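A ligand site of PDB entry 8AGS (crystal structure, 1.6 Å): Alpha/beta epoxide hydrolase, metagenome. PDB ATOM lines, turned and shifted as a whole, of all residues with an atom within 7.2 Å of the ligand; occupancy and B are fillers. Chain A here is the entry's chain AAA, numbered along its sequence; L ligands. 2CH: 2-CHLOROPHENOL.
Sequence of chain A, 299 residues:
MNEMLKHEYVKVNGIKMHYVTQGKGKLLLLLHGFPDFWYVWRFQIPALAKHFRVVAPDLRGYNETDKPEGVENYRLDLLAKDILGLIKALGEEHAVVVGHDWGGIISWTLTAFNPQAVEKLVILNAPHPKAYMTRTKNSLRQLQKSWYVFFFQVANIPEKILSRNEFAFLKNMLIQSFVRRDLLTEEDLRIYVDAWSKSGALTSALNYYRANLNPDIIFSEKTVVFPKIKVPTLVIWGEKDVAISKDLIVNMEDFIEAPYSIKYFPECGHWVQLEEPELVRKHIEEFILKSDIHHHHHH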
ATOM      1  N   GLY A  33     -21.013   7.666 -13.205  1.00  0.00           N
ATOM      2  CA  GLY A  33     -21.562   8.901 -13.776  1.00  0.00           C
ATOM      3  C   GLY A  33     -20.533  10.023 -13.818  1.00  0.00           C
ATOM      4  O   GLY A  33     -19.311   9.768 -13.917  1.00  0.00           O
ATOM      5  N   PHE A  34     -21.036  11.267 -13.793  1.00  0.00           N
ATOM      6  CA  PHE A  34     -20.133  12.410 -13.904  1.00  0.00           C
ATOM      7  C   PHE A  34     -19.750  12.872 -12.510  1.00  0.00           C
ATOM      8  O   PHE A  34     -20.609  12.970 -11.619  1.00  0.00           O
ATOM      9  CB  PHE A  34     -20.907  13.518 -14.618  1.00  0.00           C
ATOM     10  CG  PHE A  34     -20.133  14.822 -14.675  1.00  0.00           C
ATOM     11  CD1 PHE A  34     -19.168  15.004 -15.665  1.00  0.00           C
ATOM     12  CD2 PHE A  34     -20.373  15.827 -13.743  1.00  0.00           C
ATOM     13  CE1 PHE A  34     -18.542  16.248 -15.785  1.00  0.00           C
ATOM     14  CE2 PHE A  34     -19.714  17.059 -13.856  1.00  0.00           C
ATOM     15  CZ  PHE A  34     -18.769  17.218 -14.836  1.00  0.00           C
ATOM     16  N   HIS A 100     -25.067   4.482 -11.374  1.00  0.00           N
ATOM     17  CA  HIS A 100     -25.094   5.656 -10.519  1.00  0.00           C
ATOM     18  C   HIS A 100     -25.043   6.916 -11.379  1.00  0.00           C
ATOM     19  O   HIS A 100     -24.309   6.900 -12.378  1.00  0.00           O
ATOM     20  CB  HIS A 100     -23.860   5.612  -9.564  1.00  0.00           C
ATOM     21  CG  HIS A 100     -23.701   6.843  -8.732  1.00  0.00           C
ATOM     22  ND1 HIS A 100     -22.609   7.718  -8.910  1.00  0.00           N
ATOM     23  CD2 HIS A 100     -24.471   7.384  -7.776  1.00  0.00           C
ATOM     24  CE1 HIS A 100     -22.750   8.727  -8.089  1.00  0.00           C
ATOM     25  NE2 HIS A 100     -23.881   8.544  -7.368  1.00  0.00           N
ATOM     26  N   ASP A 101     -25.908   7.931 -11.073  1.00  0.00           N
ATOM     27  CA  ASP A 101     -25.791   9.211 -11.775  1.00  0.00           C
ATOM     28  C   ASP A 101     -26.077   8.974 -13.287  1.00  0.00           C
ATOM     29  O   ASP A 101     -27.002   8.264 -13.640  1.00  0.00           O
ATOM     30  CB  ASP A 101     -24.403   9.832 -11.448  1.00  0.00           C
ATOM     31  CG  ASP A 101     -24.092  11.259 -11.895  1.00  0.00           C
ATOM     32  OD1 ASP A 101     -23.743  11.499 -13.102  1.00  0.00           O
ATOM     33  OD2 ASP A 101     -24.328  12.197 -11.052  1.00  0.00           O
ATOM     34  N   TRP A 102     -25.236   9.484 -14.238  1.00  0.00           N
ATOM     35  CA  TRP A 102     -25.486   9.161 -15.629  1.00  0.00           C
ATOM     36  C   TRP A 102     -25.513   7.667 -15.921  1.00  0.00           C
ATOM     37  O   TRP A 102     -26.257   7.209 -16.781  1.00  0.00           O
ATOM     38  CB  TRP A 102     -24.412   9.808 -16.564  1.00  0.00           C
ATOM     39  CG  TRP A 102     -24.702  11.213 -16.901  1.00  0.00           C
ATOM     40  CD1 TRP A 102     -24.102  12.288 -16.330  1.00  0.00           C
ATOM     41  CD2 TRP A 102     -25.711  11.686 -17.802  1.00  0.00           C
ATOM     42  NE1 TRP A 102     -24.602  13.406 -16.888  1.00  0.00           N
ATOM     43  CE2 TRP A 102     -25.598  13.101 -17.770  1.00  0.00           C
ATOM     44  CE3 TRP A 102     -26.627  11.046 -18.644  1.00  0.00           C
ATOM     45  CZ2 TRP A 102     -26.422  13.910 -18.530  1.00  0.00           C
ATOM     46  CZ3 TRP A 102     -27.454  11.875 -19.414  1.00  0.00           C
ATOM     47  CH2 TRP A 102     -27.337  13.262 -19.335  1.00  0.00           C
ATOM     48  N   GLY A 103     -24.663   6.887 -15.220  1.00  0.00           N
ATOM     49  CA  GLY A 103     -24.684   5.455 -15.397  1.00  0.00           C
ATOM     50  C   GLY A 103     -26.082   4.907 -15.105  1.00  0.00           C
ATOM     51  O   GLY A 103     -26.499   3.948 -15.761  1.00  0.00           O
ATOM     52  N   GLY A 104     -26.725   5.487 -14.120  1.00  0.00           N
ATOM     53  CA  GLY A 104     -28.118   5.110 -13.788  1.00  0.00           C
ATOM     54  C   GLY A 104     -29.117   5.580 -14.843  1.00  0.00           C
ATOM     55  O   GLY A 104     -30.054   4.865 -15.161  1.00  0.00           O
ATOM     56  N   ILE A 105     -28.979   6.801 -15.372  1.00  0.00           N
ATOM     57  CA  ILE A 105     -29.885   7.232 -16.429  1.00  0.00           C
ATOM     58  C   ILE A 105     -29.750   6.258 -17.600  1.00  0.00           C
ATOM     59  O   ILE A 105     -30.754   5.897 -18.234  1.00  0.00           O
ATOM     60  CB  ILE A 105     -29.552   8.687 -16.822  1.00  0.00           C
ATOM     61  CG1 ILE A 105     -29.798   9.621 -15.623  1.00  0.00           C
ATOM     62  CG2 ILE A 105     -30.362   9.095 -18.066  1.00  0.00           C
ATOM     63  CD1 ILE A 105     -29.259  11.060 -15.816  1.00  0.00           C
ATOM     64  N   LEU A 124     -28.547   3.832  -8.243  1.00  0.00           N
ATOM     65  CA  LEU A 124     -28.163   4.624  -7.096  1.00  0.00           C
ATOM     66  C   LEU A 124     -28.238   6.096  -7.506  1.00  0.00           C
ATOM     67  O   LEU A 124     -27.572   6.512  -8.470  1.00  0.00           O
ATOM     68  CB  LEU A 124     -26.687   4.309  -6.772  1.00  0.00           C
ATOM     69  CG  LEU A 124     -26.371   3.068  -5.926  1.00  0.00           C
ATOM     70  CD1 LEU A 124     -26.701   1.844  -6.708  1.00  0.00           C
ATOM     71  CD2 LEU A 124     -24.808   3.085  -5.704  1.00  0.00           C
ATOM     72  N   ASN A 125     -29.097   6.878  -6.844  1.00  0.00           N
ATOM     73  CA  ASN A 125     -29.132   8.336  -7.046  1.00  0.00           C
ATOM     74  C   ASN A 125     -29.043   8.728  -8.532  1.00  0.00           C
ATOM     75  O   ASN A 125     -28.182   9.534  -8.969  1.00  0.00           O
ATOM     76  CB  ASN A 125     -28.031   9.021  -6.222  1.00  0.00           C
ATOM     77  CG  ASN A 125     -28.428   9.025  -4.745  1.00  0.00           C
ATOM     78  OD1 ASN A 125     -28.225   8.031  -4.041  1.00  0.00           O
ATOM     79  ND2 ASN A 125     -28.923  10.159  -4.257  1.00  0.00           N
ATOM     80  N   ALA A 126     -30.028   8.275  -9.298  1.00  0.00           N
ATOM     81  CA  ALA A 126     -30.172   8.678 -10.693  1.00  0.00           C
ATOM     82  C   ALA A 126     -31.656   8.772 -10.911  1.00  0.00           C
ATOM     83  O   ALA A 126     -32.375   7.792 -10.686  1.00  0.00           O
ATOM     84  CB  ALA A 126     -29.600   7.675 -11.676  1.00  0.00           C
ATOM     85  N   PRO A 127     -32.142   9.969 -11.329  1.00  0.00           N
ATOM     86  CA  PRO A 127     -33.576  10.122 -11.585  1.00  0.00           C
ATOM     87  C   PRO A 127     -33.970   9.273 -12.805  1.00  0.00           C
ATOM     88  O   PRO A 127     -33.199   9.107 -13.731  1.00  0.00           O
ATOM     89  CB  PRO A 127     -33.724  11.616 -11.951  1.00  0.00           C
ATOM     90  CG  PRO A 127     -32.368  11.971 -12.518  1.00  0.00           C
ATOM     91  CD  PRO A 127     -31.336  11.160 -11.742  1.00  0.00           C
ATOM     92  N   TYR A 132     -37.326  13.175 -14.768  1.00  0.00           N
ATOM     93  CA  TYR A 132     -36.532  14.382 -14.967  1.00  0.00           C
ATOM     94  C   TYR A 132     -37.165  15.240 -16.068  1.00  0.00           C
ATOM     95  O   TYR A 132     -37.390  16.426 -15.843  1.00  0.00           O
ATOM     96  CB  TYR A 132     -35.067  14.094 -15.299  1.00  0.00           C
ATOM     97  CG  TYR A 132     -34.204  15.337 -15.204  1.00  0.00           C
ATOM     98  CD1 TYR A 132     -34.153  16.256 -16.244  1.00  0.00           C
ATOM     99  CD2 TYR A 132     -33.497  15.647 -14.052  1.00  0.00           C
ATOM    100  CE1 TYR A 132     -33.371  17.412 -16.152  1.00  0.00           C
ATOM    101  CE2 TYR A 132     -32.727  16.790 -13.943  1.00  0.00           C
ATOM    102  CZ  TYR A 132     -32.679  17.687 -14.995  1.00  0.00           C
ATOM    103  OH  TYR A 132     -31.935  18.847 -14.950  1.00  0.00           O
ATOM    104  N   GLN A 142     -35.603  21.669  -8.287  1.00  0.00           N
ATOM    105  CA  GLN A 142     -34.762  20.926  -9.245  1.00  0.00           C
ATOM    106  C   GLN A 142     -34.056  21.877 -10.210  1.00  0.00           C
ATOM    107  O   GLN A 142     -32.890  21.637 -10.572  1.00  0.00           O
ATOM    108  CB  GLN A 142     -35.551  19.897 -10.064  1.00  0.00           C
ATOM    109  CG  GLN A 142     -34.697  19.004 -10.995  1.00  0.00           C
ATOM    110  CD  GLN A 142     -33.686  18.242 -10.143  1.00  0.00           C
ATOM    111  OE1 GLN A 142     -34.044  17.554  -9.209  1.00  0.00           O
ATOM    112  NE2 GLN A 142     -32.371  18.371 -10.380  1.00  0.00           N
ATOM    113  N   SER A 146     -30.076  22.025 -10.650  1.00  0.00           N
ATOM    114  CA  SER A 146     -29.508  21.822 -11.972  1.00  0.00           C
ATOM    115  C   SER A 146     -28.853  23.069 -12.560  1.00  0.00           C
ATOM    116  O   SER A 146     -28.675  23.134 -13.764  1.00  0.00           O
ATOM    117  CB  SER A 146     -30.559  21.226 -12.904  1.00  0.00           C
ATOM    118  OG  SER A 146     -30.864  19.884 -12.509  1.00  0.00           O
ATOM    119  N   TYR A 148     -25.846  23.737 -12.812  1.00  0.00           N
ATOM    120  CA  TYR A 148     -24.633  23.406 -13.562  1.00  0.00           C
ATOM    121  C   TYR A 148     -24.999  22.730 -14.875  1.00  0.00           C
ATOM    122  O   TYR A 148     -24.222  22.782 -15.828  1.00  0.00           O
ATOM    123  CB  TYR A 148     -23.720  22.514 -12.694  1.00  0.00           C
ATOM    124  CG  TYR A 148     -24.334  21.178 -12.374  1.00  0.00           C
ATOM    125  CD1 TYR A 148     -25.195  21.027 -11.286  1.00  0.00           C
ATOM    126  CD2 TYR A 148     -24.121  20.078 -13.217  1.00  0.00           C
ATOM    127  CE1 TYR A 148     -25.838  19.817 -11.016  1.00  0.00           C
ATOM    128  CE2 TYR A 148     -24.739  18.855 -12.929  1.00  0.00           C
ATOM    129  CZ  TYR A 148     -25.633  18.744 -11.872  1.00  0.00           C
ATOM    130  OH  TYR A 148     -26.269  17.547 -11.642  1.00  0.00           O
ATOM    131  N   VAL A 149     -26.213  22.107 -14.954  1.00  0.00           N
ATOM    132  CA  VAL A 149     -26.656  21.571 -16.247  1.00  0.00           C
ATOM    133  C   VAL A 149     -26.777  22.701 -17.281  1.00  0.00           C
ATOM    134  O   VAL A 149     -26.404  22.522 -18.431  1.00  0.00           O
ATOM    135  CB  VAL A 149     -28.049  20.884 -16.110  1.00  0.00           C
ATOM    136  CG1 VAL A 149     -28.597  20.385 -17.446  1.00  0.00           C
ATOM    137  CG2 VAL A 149     -27.974  19.711 -15.123  1.00  0.00           C
ATOM    138  N   PHE A 152     -23.269  24.036 -18.288  1.00  0.00           N
ATOM    139  CA  PHE A 152     -22.550  23.109 -19.172  1.00  0.00           C
ATOM    140  C   PHE A 152     -23.012  23.232 -20.638  1.00  0.00           C
ATOM    141  O   PHE A 152     -22.391  22.636 -21.516  1.00  0.00           O
ATOM    142  CB  PHE A 152     -22.740  21.659 -18.678  1.00  0.00           C
ATOM    143  CG  PHE A 152     -22.009  21.322 -17.392  1.00  0.00           C
ATOM    144  CD1 PHE A 152     -21.138  22.239 -16.785  1.00  0.00           C
ATOM    145  CD2 PHE A 152     -22.195  20.073 -16.795  1.00  0.00           C
ATOM    146  CE1 PHE A 152     -20.462  21.880 -15.622  1.00  0.00           C
ATOM    147  CE2 PHE A 152     -21.531  19.738 -15.623  1.00  0.00           C
ATOM    148  CZ  PHE A 152     -20.651  20.647 -15.044  1.00  0.00           C
ATOM    149  N   TYR A 209     -24.566  16.254 -21.264  1.00  0.00           N
ATOM    150  CA  TYR A 209     -25.530  17.256 -20.865  1.00  0.00           C
ATOM    151  C   TYR A 209     -26.098  18.016 -22.074  1.00  0.00           C
ATOM    152  O   TYR A 209     -27.289  18.366 -22.098  1.00  0.00           O
ATOM    153  CB  TYR A 209     -24.858  18.243 -19.906  1.00  0.00           C
ATOM    154  CG  TYR A 209     -24.514  17.585 -18.595  1.00  0.00           C
ATOM    155  CD1 TYR A 209     -23.266  16.994 -18.443  1.00  0.00           C
ATOM    156  CD2 TYR A 209     -25.399  17.607 -17.525  1.00  0.00           C
ATOM    157  CE1 TYR A 209     -22.922  16.391 -17.236  1.00  0.00           C
ATOM    158  CE2 TYR A 209     -25.067  16.986 -16.310  1.00  0.00           C
ATOM    159  CZ  TYR A 209     -23.843  16.359 -16.196  1.00  0.00           C
ATOM    160  OH  TYR A 209     -23.543  15.742 -15.005  1.00  0.00           O
ATOM    161  N   LEU A 213     -29.808  17.022 -22.099  1.00  0.00           N
ATOM    162  CA  LEU A 213     -30.420  17.833 -21.069  1.00  0.00           C
ATOM    163  C   LEU A 213     -30.333  19.314 -21.480  1.00  0.00           C
ATOM    164  O   LEU A 213     -30.304  20.212 -20.624  1.00  0.00           O
ATOM    165  CB  LEU A 213     -29.728  17.641 -19.699  1.00  0.00           C
ATOM    166  CG  LEU A 213     -29.905  16.280 -19.048  1.00  0.00           C
ATOM    167  CD1 LEU A 213     -29.092  16.194 -17.748  1.00  0.00           C
ATOM    168  CD2 LEU A 213     -31.376  15.886 -18.820  1.00  0.00           C
ATOM    169  N   ASP A 241     -28.925  14.675  -1.334  1.00  0.00           N
ATOM    170  CA  ASP A 241     -28.402  14.790  -2.700  1.00  0.00           C
ATOM    171  C   ASP A 241     -28.456  16.263  -3.165  1.00  0.00           C
ATOM    172  O   ASP A 241     -29.535  16.831  -3.314  1.00  0.00           O
ATOM    173  CB  ASP A 241     -29.301  13.947  -3.654  1.00  0.00           C
ATOM    174  CG  ASP A 241     -28.644  13.707  -4.992  1.00  0.00           C
ATOM    175  OD1 ASP A 241     -28.057  14.681  -5.548  1.00  0.00           O
ATOM    176  OD2 ASP A 241     -28.709  12.540  -5.508  1.00  0.00           O
ATOM    177  N   ALA A 243     -27.780  17.368  -6.058  1.00  0.00           N
ATOM    178  CA  ALA A 243     -28.097  17.488  -7.476  1.00  0.00           C
ATOM    179  C   ALA A 243     -29.516  17.105  -7.840  1.00  0.00           C
ATOM    180  O   ALA A 243     -29.964  17.463  -8.909  1.00  0.00           O
ATOM    181  CB  ALA A 243     -27.144  16.624  -8.330  1.00  0.00           C
ATOM    182  N   ILE A 244     -30.195  16.323  -6.978  1.00  0.00           N
ATOM    183  CA  ILE A 244     -31.515  15.806  -7.354  1.00  0.00           C
ATOM    184  C   ILE A 244     -32.500  16.140  -6.235  1.00  0.00           C
ATOM    185  O   ILE A 244     -32.279  15.734  -5.093  1.00  0.00           O
ATOM    186  CB  ILE A 244     -31.452  14.274  -7.615  1.00  0.00           C
ATOM    187  CG1 ILE A 244     -30.345  13.929  -8.615  1.00  0.00           C
ATOM    188  CG2 ILE A 244     -32.817  13.771  -8.087  1.00  0.00           C
ATOM    189  CD1 ILE A 244     -29.933  12.394  -8.691  1.00  0.00           C
ATOM    190  N   LEU A 248     -38.316  14.722  -7.773  1.00  0.00           N
ATOM    191  CA  LEU A 248     -38.145  13.843  -8.912  1.00  0.00           C
ATOM    192  C   LEU A 248     -38.300  12.361  -8.536  1.00  0.00           C
ATOM    193  O   LEU A 248     -38.324  11.521  -9.420  1.00  0.00           O
ATOM    194  CB  LEU A 248     -36.755  14.068  -9.549  1.00  0.00           C
ATOM    195  CG  LEU A 248     -36.804  15.071 -10.731  1.00  0.00           C
ATOM    196  CD1 LEU A 248     -37.439  16.396 -10.348  1.00  0.00           C
ATOM    197  CD2 LEU A 248     -35.425  15.233 -11.371  1.00  0.00           C
ATOM    198  N   HIS A 270     -25.346  12.260  -2.713  1.00  0.00           N
ATOM    199  CA  HIS A 270     -25.403  11.749  -4.066  1.00  0.00           C
ATOM    200  C   HIS A 270     -24.459  10.559  -4.197  1.00  0.00           C
ATOM    201  O   HIS A 270     -24.765   9.626  -4.964  1.00  0.00           O
ATOM    202  CB  HIS A 270     -25.001  12.893  -5.030  1.00  0.00           C
ATOM    203  CG  HIS A 270     -25.183  12.555  -6.469  1.00  0.00           C
ATOM    204  ND1 HIS A 270     -26.459  12.326  -7.027  1.00  0.00           N
ATOM    205  CD2 HIS A 270     -24.269  12.341  -7.458  1.00  0.00           C
ATOM    206  CE1 HIS A 270     -26.300  12.046  -8.310  1.00  0.00           C
ATOM    207  NE2 HIS A 270     -24.982  12.043  -8.605  1.00  0.00           N
HETATM  208  C1  2CH L   1     -26.426  14.156 -13.510  1.00  0.00           C
HETATM  209  C2  2CH L   1     -27.533  14.455 -14.541  1.00  0.00           C
HETATM  210  C3  2CH L   1     -28.485  15.497 -13.917  1.00  0.00           C
HETATM  211  C4  2CH L   1     -29.231  14.761 -12.756  1.00  0.00           C
HETATM  212  C5  2CH L   1     -28.147  14.600 -11.681  1.00  0.00           C
HETATM  213  C6  2CH L   1     -27.055  13.666 -12.210  1.00  0.00           C
HETATM  214  O   2CH L   1     -25.650  15.401 -13.284  1.00  0.00           O
HETATM  215 CL8  2CH L   1     -27.741  12.027 -12.478  1.00  0.00          CL
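OD2 of Asp 101 touches C6 of the ligand, at 3.3 Å. Trp 102 touches the ligand (NE1 to C2, 3.9 Å). CD1 of Ile 105 touches CL8 of the ligand, at 3.8 Å. CD of Pro 127 touches CL8 of the ligand, 3.8 Å away. CD1 of Leu 213 touches C3 of the ligand (3.9 Å). CG1 of Ile 244 touches C5 of the ligand, at 3.8 Å. Hydrophobic or aromatic side chains that line the ligand: Ile 105, Pro 127, Tyr 148, Tyr 209, Leu 213 and Ile 244. Eight residues have an atom within 4 Å of the ligand: Asp 101, Trp 102, Ile 105, Pro 127, Tyr 148, Tyr 209, Leu 213 and Ile 244. The nearest printed residue that does not touch the ligand is Ala 243 (4.04 Å).
The side-chain hydroxyl of Tyr 148 is in hydrogen-bond range of an oxygen (O) of the ligand (2.8 Å). The side-chain hydroxyl (OH) of Tyr 209 is in hydrogen-bond range of an oxygen (O) of the ligand, at 2.7 Å.
The side-chain carboxylate (OD1) of Asp 241 sits at hydrogen-bond distance from the backbone NH (N) of Ile 244. The backbone carbonyl oxygen (O) of Leu 124 is in hydrogen-bond range of the backbone NH (N) of Asp 101, 3.4 Å away. The side-chain carboxylate (OD1) of Asp 101 lies within hydrogen-bond range of the backbone NH (N) of Phe 34 (2.8 Å). OD2 of Asp 101 lies within hydrogen-bond range of NE2 of His 270 (2.5 Å). N of Asp 101 is in hydrogen-bond range of O of Asn 125 (3.5 Å). NE1 of Trp 102 lies close to OH of Tyr 209 (3.2 Å).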
